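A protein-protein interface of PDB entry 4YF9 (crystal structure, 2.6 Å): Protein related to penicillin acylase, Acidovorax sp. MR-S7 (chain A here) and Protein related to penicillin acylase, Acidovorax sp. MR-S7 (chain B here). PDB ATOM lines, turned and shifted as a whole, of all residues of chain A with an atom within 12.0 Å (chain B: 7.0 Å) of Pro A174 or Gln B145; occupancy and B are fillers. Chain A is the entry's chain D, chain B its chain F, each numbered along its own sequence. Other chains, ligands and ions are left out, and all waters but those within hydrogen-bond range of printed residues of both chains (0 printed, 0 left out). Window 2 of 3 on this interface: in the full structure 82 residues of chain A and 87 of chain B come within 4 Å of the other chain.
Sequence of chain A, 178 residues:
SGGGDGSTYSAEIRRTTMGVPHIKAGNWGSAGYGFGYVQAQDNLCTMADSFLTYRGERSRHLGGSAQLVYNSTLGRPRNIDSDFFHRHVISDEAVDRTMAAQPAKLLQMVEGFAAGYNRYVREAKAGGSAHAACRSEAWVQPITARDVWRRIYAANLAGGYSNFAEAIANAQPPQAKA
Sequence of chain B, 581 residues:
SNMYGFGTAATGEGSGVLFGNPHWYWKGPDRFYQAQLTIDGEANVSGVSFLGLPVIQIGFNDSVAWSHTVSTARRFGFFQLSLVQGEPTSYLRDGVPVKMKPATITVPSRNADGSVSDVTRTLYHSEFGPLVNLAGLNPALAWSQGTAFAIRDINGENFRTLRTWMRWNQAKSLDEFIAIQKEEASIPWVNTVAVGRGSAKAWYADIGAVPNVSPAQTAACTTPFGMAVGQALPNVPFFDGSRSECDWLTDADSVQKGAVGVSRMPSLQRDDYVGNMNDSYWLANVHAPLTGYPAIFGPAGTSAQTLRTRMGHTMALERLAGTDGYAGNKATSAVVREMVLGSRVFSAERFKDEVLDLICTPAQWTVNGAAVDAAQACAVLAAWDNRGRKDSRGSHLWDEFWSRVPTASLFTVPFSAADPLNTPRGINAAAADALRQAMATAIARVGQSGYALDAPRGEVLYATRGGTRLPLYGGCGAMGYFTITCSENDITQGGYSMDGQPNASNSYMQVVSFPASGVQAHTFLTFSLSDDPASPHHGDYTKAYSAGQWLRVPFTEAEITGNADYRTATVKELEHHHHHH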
ATOM      1  N   ASN A 170     -24.450  31.319  37.535  1.00  0.00           N
ATOM      2  CA  ASN A 170     -22.996  31.395  37.452  1.00  0.00           C
ATOM      3  C   ASN A 170     -22.427  30.839  36.152  1.00  0.00           C
ATOM      4  O   ASN A 170     -21.229  30.561  36.056  1.00  0.00           O
ATOM      5  CB  ASN A 170     -22.354  30.716  38.663  1.00  0.00           C
ATOM      6  CG  ASN A 170     -22.621  31.463  39.957  1.00  0.00           C
ATOM      7  OD1 ASN A 170     -21.835  32.316  40.371  1.00  0.00           O
ATOM      8  ND2 ASN A 170     -23.747  31.162  40.592  1.00  0.00           N
ATOM      9  N   ALA A 171     -23.288  30.697  35.150  1.00  0.00           N
ATOM     10  CA  ALA A 171     -22.858  30.243  33.832  1.00  0.00           C
ATOM     11  C   ALA A 171     -22.326  31.396  32.982  1.00  0.00           C
ATOM     12  O   ALA A 171     -23.107  32.155  32.387  1.00  0.00           O
ATOM     13  CB  ALA A 171     -23.999  29.545  33.119  1.00  0.00           C
ATOM     14  N   GLN A 172     -21.000  31.526  32.940  1.00  0.00           N
ATOM     15  CA  GLN A 172     -20.324  32.514  32.087  1.00  0.00           C
ATOM     16  C   GLN A 172     -19.012  31.977  31.516  1.00  0.00           C
ATOM     17  O   GLN A 172     -18.346  31.169  32.163  1.00  0.00           O
ATOM     18  CB  GLN A 172     -20.092  33.828  32.828  1.00  0.00           C
ATOM     19  CG  GLN A 172     -19.797  33.681  34.307  1.00  0.00           C
ATOM     20  CD  GLN A 172     -20.540  34.725  35.113  1.00  0.00           C
ATOM     21  OE1 GLN A 172     -20.149  35.889  35.153  1.00  0.00           O
ATOM     22  NE2 GLN A 172     -21.632  34.312  35.747  1.00  0.00           N
ATOM     23  N   PRO A 173     -18.644  32.422  30.296  1.00  0.00           N
ATOM     24  CA  PRO A 173     -17.459  31.935  29.571  1.00  0.00           C
ATOM     25  C   PRO A 173     -16.119  32.212  30.283  1.00  0.00           C
ATOM     26  O   PRO A 173     -16.090  32.973  31.251  1.00  0.00           O
ATOM     27  CB  PRO A 173     -17.533  32.698  28.241  1.00  0.00           C
ATOM     28  CG  PRO A 173     -18.332  33.919  28.539  1.00  0.00           C
ATOM     29  CD  PRO A 173     -19.356  33.466  29.530  1.00  0.00           C
ATOM     30  N   PRO A 174     -15.018  31.587  29.815  1.00  0.00           N
ATOM     31  CA  PRO A 174     -13.696  31.863  30.395  1.00  0.00           C
ATOM     32  C   PRO A 174     -13.112  33.225  29.991  1.00  0.00           C
ATOM     33  O   PRO A 174     -13.558  33.831  29.019  1.00  0.00           O
ATOM     34  CB  PRO A 174     -12.827  30.728  29.844  1.00  0.00           C
ATOM     35  CG  PRO A 174     -13.500  30.312  28.582  1.00  0.00           C
ATOM     36  CD  PRO A 174     -14.970  30.491  28.827  1.00  0.00           C
ATOM     37  N   SER B  82     -20.958  22.779  21.220  1.00  0.00           N
ATOM     38  CA  SER B  82     -19.638  22.884  20.621  1.00  0.00           C
ATOM     39  C   SER B  82     -19.391  24.334  20.248  1.00  0.00           C
ATOM     40  O   SER B  82     -19.999  24.870  19.314  1.00  0.00           O
ATOM     41  CB  SER B  82     -19.511  21.970  19.401  1.00  0.00           C
ATOM     42  OG  SER B  82     -19.563  20.612  19.793  1.00  0.00           O
ATOM     43  N   LEU B  83     -18.498  24.963  21.001  1.00  0.00           N
ATOM     44  CA  LEU B  83     -18.229  26.390  20.869  1.00  0.00           C
ATOM     45  C   LEU B  83     -17.362  26.726  19.663  1.00  0.00           C
ATOM     46  O   LEU B  83     -16.446  25.980  19.320  1.00  0.00           O
ATOM     47  CB  LEU B  83     -17.576  26.919  22.150  1.00  0.00           C
ATOM     48  CG  LEU B  83     -18.303  26.646  23.470  1.00  0.00           C
ATOM     49  CD1 LEU B  83     -17.475  27.163  24.632  1.00  0.00           C
ATOM     50  CD2 LEU B  83     -19.687  27.274  23.464  1.00  0.00           C
ATOM     51  N   VAL B  84     -17.670  27.858  19.032  1.00  0.00           N
ATOM     52  CA  VAL B  84     -16.868  28.420  17.941  1.00  0.00           C
ATOM     53  C   VAL B  84     -15.502  28.827  18.480  1.00  0.00           C
ATOM     54  O   VAL B  84     -15.410  29.498  19.506  1.00  0.00           O
ATOM     55  CB  VAL B  84     -17.569  29.648  17.308  1.00  0.00           C
ATOM     56  CG1 VAL B  84     -16.697  30.300  16.238  1.00  0.00           C
ATOM     57  CG2 VAL B  84     -18.917  29.250  16.727  1.00  0.00           C
ATOM     58  N   GLN B  85     -14.443  28.406  17.791  1.00  0.00           N
ATOM     59  CA  GLN B  85     -13.086  28.737  18.206  1.00  0.00           C
ATOM     60  C   GLN B  85     -12.897  30.255  18.182  1.00  0.00           C
ATOM     61  O   GLN B  85     -13.266  30.917  17.209  1.00  0.00           O
ATOM     62  CB  GLN B  85     -12.065  28.045  17.308  1.00  0.00           C
ATOM     63  CG  GLN B  85     -10.865  27.499  18.063  1.00  0.00           C
ATOM     64  CD  GLN B  85      -9.550  27.988  17.486  1.00  0.00           C
ATOM     65  OE1 GLN B  85      -8.998  28.987  17.951  1.00  0.00           O
ATOM     66  NE2 GLN B  85      -9.047  27.299  16.456  1.00  0.00           N
ATOM     67  N   GLY B  86     -12.356  30.799  19.273  1.00  0.00           N
ATOM     68  CA  GLY B  86     -12.195  32.248  19.442  1.00  0.00           C
ATOM     69  C   GLY B  86     -13.404  32.949  20.052  1.00  0.00           C
ATOM     70  O   GLY B  86     -13.279  34.043  20.610  1.00  0.00           O
ATOM     71  N   GLU B  87     -14.570  32.310  19.959  1.00  0.00           N
ATOM     72  CA  GLU B  87     -15.842  32.912  20.354  1.00  0.00           C
ATOM     73  C   GLU B  87     -16.596  32.044  21.370  1.00  0.00           C
ATOM     74  O   GLU B  87     -17.522  31.317  20.998  1.00  0.00           O
ATOM     75  CB  GLU B  87     -16.701  33.140  19.106  1.00  0.00           C
ATOM     76  CG  GLU B  87     -17.773  34.209  19.256  1.00  0.00           C
ATOM     77  CD  GLU B  87     -18.268  34.719  17.916  1.00  0.00           C
ATOM     78  OE1 GLU B  87     -19.497  34.711  17.692  1.00  0.00           O
ATOM     79  OE2 GLU B  87     -17.427  35.121  17.082  1.00  0.00           O
ATOM     80  N   PRO B  88     -16.212  32.127  22.663  1.00  0.00           N
ATOM     81  CA  PRO B  88     -16.797  31.247  23.687  1.00  0.00           C
ATOM     82  C   PRO B  88     -18.272  31.524  24.041  1.00  0.00           C
ATOM     83  O   PRO B  88     -18.796  30.915  24.974  1.00  0.00           O
ATOM     84  CB  PRO B  88     -15.885  31.466  24.905  1.00  0.00           C
ATOM     85  CG  PRO B  88     -15.306  32.823  24.710  1.00  0.00           C
ATOM     86  CD  PRO B  88     -15.167  33.010  23.223  1.00  0.00           C
ATOM     87  N   SER B  90     -20.563  31.589  21.326  1.00  0.00           N
ATOM     88  CA  SER B  90     -21.256  31.088  20.140  1.00  0.00           C
ATOM     89  C   SER B  90     -21.108  29.576  20.012  1.00  0.00           C
ATOM     90  O   SER B  90     -20.058  29.019  20.340  1.00  0.00           O
ATOM     91  CB  SER B  90     -20.752  31.784  18.878  1.00  0.00           C
ATOM     92  OG  SER B  90     -21.399  33.032  18.710  1.00  0.00           O
ATOM     93  N   ALA B 142     -16.603  22.170  33.114  1.00  0.00           N
ATOM     94  CA  ALA B 142     -16.564  23.627  33.153  1.00  0.00           C
ATOM     95  C   ALA B 142     -16.886  24.203  31.781  1.00  0.00           C
ATOM     96  O   ALA B 142     -16.873  23.489  30.782  1.00  0.00           O
ATOM     97  CB  ALA B 142     -15.197  24.104  33.622  1.00  0.00           C
ATOM     98  N   TRP B 143     -17.196  25.495  31.737  1.00  0.00           N
ATOM     99  CA  TRP B 143     -17.363  26.190  30.471  1.00  0.00           C
ATOM    100  C   TRP B 143     -15.984  26.575  29.968  1.00  0.00           C
ATOM    101  O   TRP B 143     -15.330  27.469  30.507  1.00  0.00           O
ATOM    102  CB  TRP B 143     -18.286  27.387  30.661  1.00  0.00           C
ATOM    103  CG  TRP B 143     -18.633  28.183  29.419  1.00  0.00           C
ATOM    104  CD1 TRP B 143     -17.951  28.234  28.197  1.00  0.00           C
ATOM    105  CD2 TRP B 143     -19.742  29.137  29.268  1.00  0.00           C
ATOM    106  NE1 TRP B 143     -18.561  29.107  27.328  1.00  0.00           N
ATOM    107  CE2 TRP B 143     -19.639  29.681  27.905  1.00  0.00           C
ATOM    108  CE3 TRP B 143     -20.779  29.565  30.089  1.00  0.00           C
ATOM    109  CZ2 TRP B 143     -20.540  30.612  27.419  1.00  0.00           C
ATOM    110  CZ3 TRP B 143     -21.683  30.509  29.584  1.00  0.00           C
ATOM    111  CH2 TRP B 143     -21.564  31.017  28.282  1.00  0.00           C
ATOM    112  N   SER B 144     -15.528  25.870  28.937  1.00  0.00           N
ATOM    113  CA  SER B 144     -14.162  25.998  28.448  1.00  0.00           C
ATOM    114  C   SER B 144     -14.117  26.701  27.101  1.00  0.00           C
ATOM    115  O   SER B 144     -15.096  27.324  26.684  1.00  0.00           O
ATOM    116  CB  SER B 144     -13.510  24.615  28.334  1.00  0.00           C
ATOM    117  OG  SER B 144     -14.222  23.797  27.421  1.00  0.00           O
ATOM    118  N   GLN B 145     -12.976  26.585  26.427  1.00  0.00           N
ATOM    119  CA  GLN B 145     -12.771  27.201  25.125  1.00  0.00           C
ATOM    120  C   GLN B 145     -13.638  26.570  24.043  1.00  0.00           C
ATOM    121  O   GLN B 145     -14.084  27.253  23.115  1.00  0.00           O
ATOM    122  CB  GLN B 145     -11.296  27.124  24.726  1.00  0.00           C
ATOM    123  CG  GLN B 145     -10.832  28.319  23.909  1.00  0.00           C
ATOM    124  CD  GLN B 145     -11.155  29.640  24.594  1.00  0.00           C
ATOM    125  OE1 GLN B 145     -10.976  29.784  25.806  1.00  0.00           O
ATOM    126  NE2 GLN B 145     -11.643  30.604  23.821  1.00  0.00           N
ATOM    127  N   GLY B 146     -13.882  25.269  24.182  1.00  0.00           N
ATOM    128  CA  GLY B 146     -14.614  24.500  23.184  1.00  0.00           C
ATOM    129  C   GLY B 146     -15.928  23.893  23.632  1.00  0.00           C
ATOM    130  O   GLY B 146     -16.687  23.399  22.802  1.00  0.00           O
ATOM    131  N   THR B 147     -16.214  23.931  24.932  1.00  0.00           N
ATOM    132  CA  THR B 147     -17.420  23.279  25.457  1.00  0.00           C
ATOM    133  C   THR B 147     -18.219  24.165  26.427  1.00  0.00           C
ATOM    134  O   THR B 147     -17.641  24.917  27.217  1.00  0.00           O
ATOM    135  CB  THR B 147     -17.077  21.920  26.114  1.00  0.00           C
ATOM    136  OG1 THR B 147     -16.229  21.166  25.239  1.00  0.00           O
ATOM    137  CG2 THR B 147     -18.332  21.111  26.398  1.00  0.00           C
ATOM    138  N   ALA B 148     -19.549  24.073  26.341  1.00  0.00           N
ATOM    139  CA  ALA B 148     -20.470  24.768  27.246  1.00  0.00           C
ATOM    140  C   ALA B 148     -21.767  23.966  27.405  1.00  0.00           C
ATOM    141  O   ALA B 148     -21.987  22.990  26.677  1.00  0.00           O
ATOM    142  CB  ALA B 148     -20.763  26.169  26.737  1.00  0.00           C
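Hydrophobic or aromatic side chains of chain B that line the printed part of chain A: Pro B88 and Trp B143. Hydrophobic or aromatic side chains of chain A that line the printed part of chain B: Pro A173 and Pro A174. Among the printed residues, no Asp or Glu carboxylate lies within 4 Å of a Lys or Arg side-chain nitrogen of the other chain.
Trp B143 touches Ala A171. Trp B143 touches Gln A172 (CE3 to C, 3.3 Å). Pro B88 touches Pro A173. Pro A173 touches Trp B143 (CD to CH2, 3.5 Å). Trp B143 touches Pro A174 (O to CD, 3.5 Å). Ser B144 touches Pro A174 (O to CD, 3.8 Å). CG of Pro A174 touches OE1 of Gln B145, 3.8 Å away.
Pro A174 touches just these residues of chain B: Trp B143 (3.5 Å), Ser B144 (3.8 Å) and Gln B145 (3.8 Å). Gln B145 touches one residue of chain A. No residue of chain A comes within 4 Å of Leu B83. No residue of chain A comes within 4 Å of Gln B85. No residue of chain A comes within 4 Å of Gly B86. Pro B88 touches just one residue of chain A: Pro A173. Trp B143 touches just these residues of chain A: Ala A171, Gln A172, Pro A173 and Pro A174. Of the printed residues of chain A, Ser B144 touches Pro A174 (3.8 Å). Of the printed residues of chain B, Gln A172 touches Trp B143 (3.3 Å). Printed residues of chain B within 4 Å of Ala A171: Trp B143. Printed residues of chain B within 4 Å of Pro A173: Pro B88 (3.9 Å) and Trp B143 (3.5 Å). Ser B82 touches none of the printed residues of chain A.
OG of Ser B144 sits at hydrogen-bond distance from N of Thr B147, at 3.2 Å. The backbone carbonyl oxygen of Pro B88 sits at hydrogen-bond distance from the indole nitrogen of Trp B143, at 3.0 Å.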
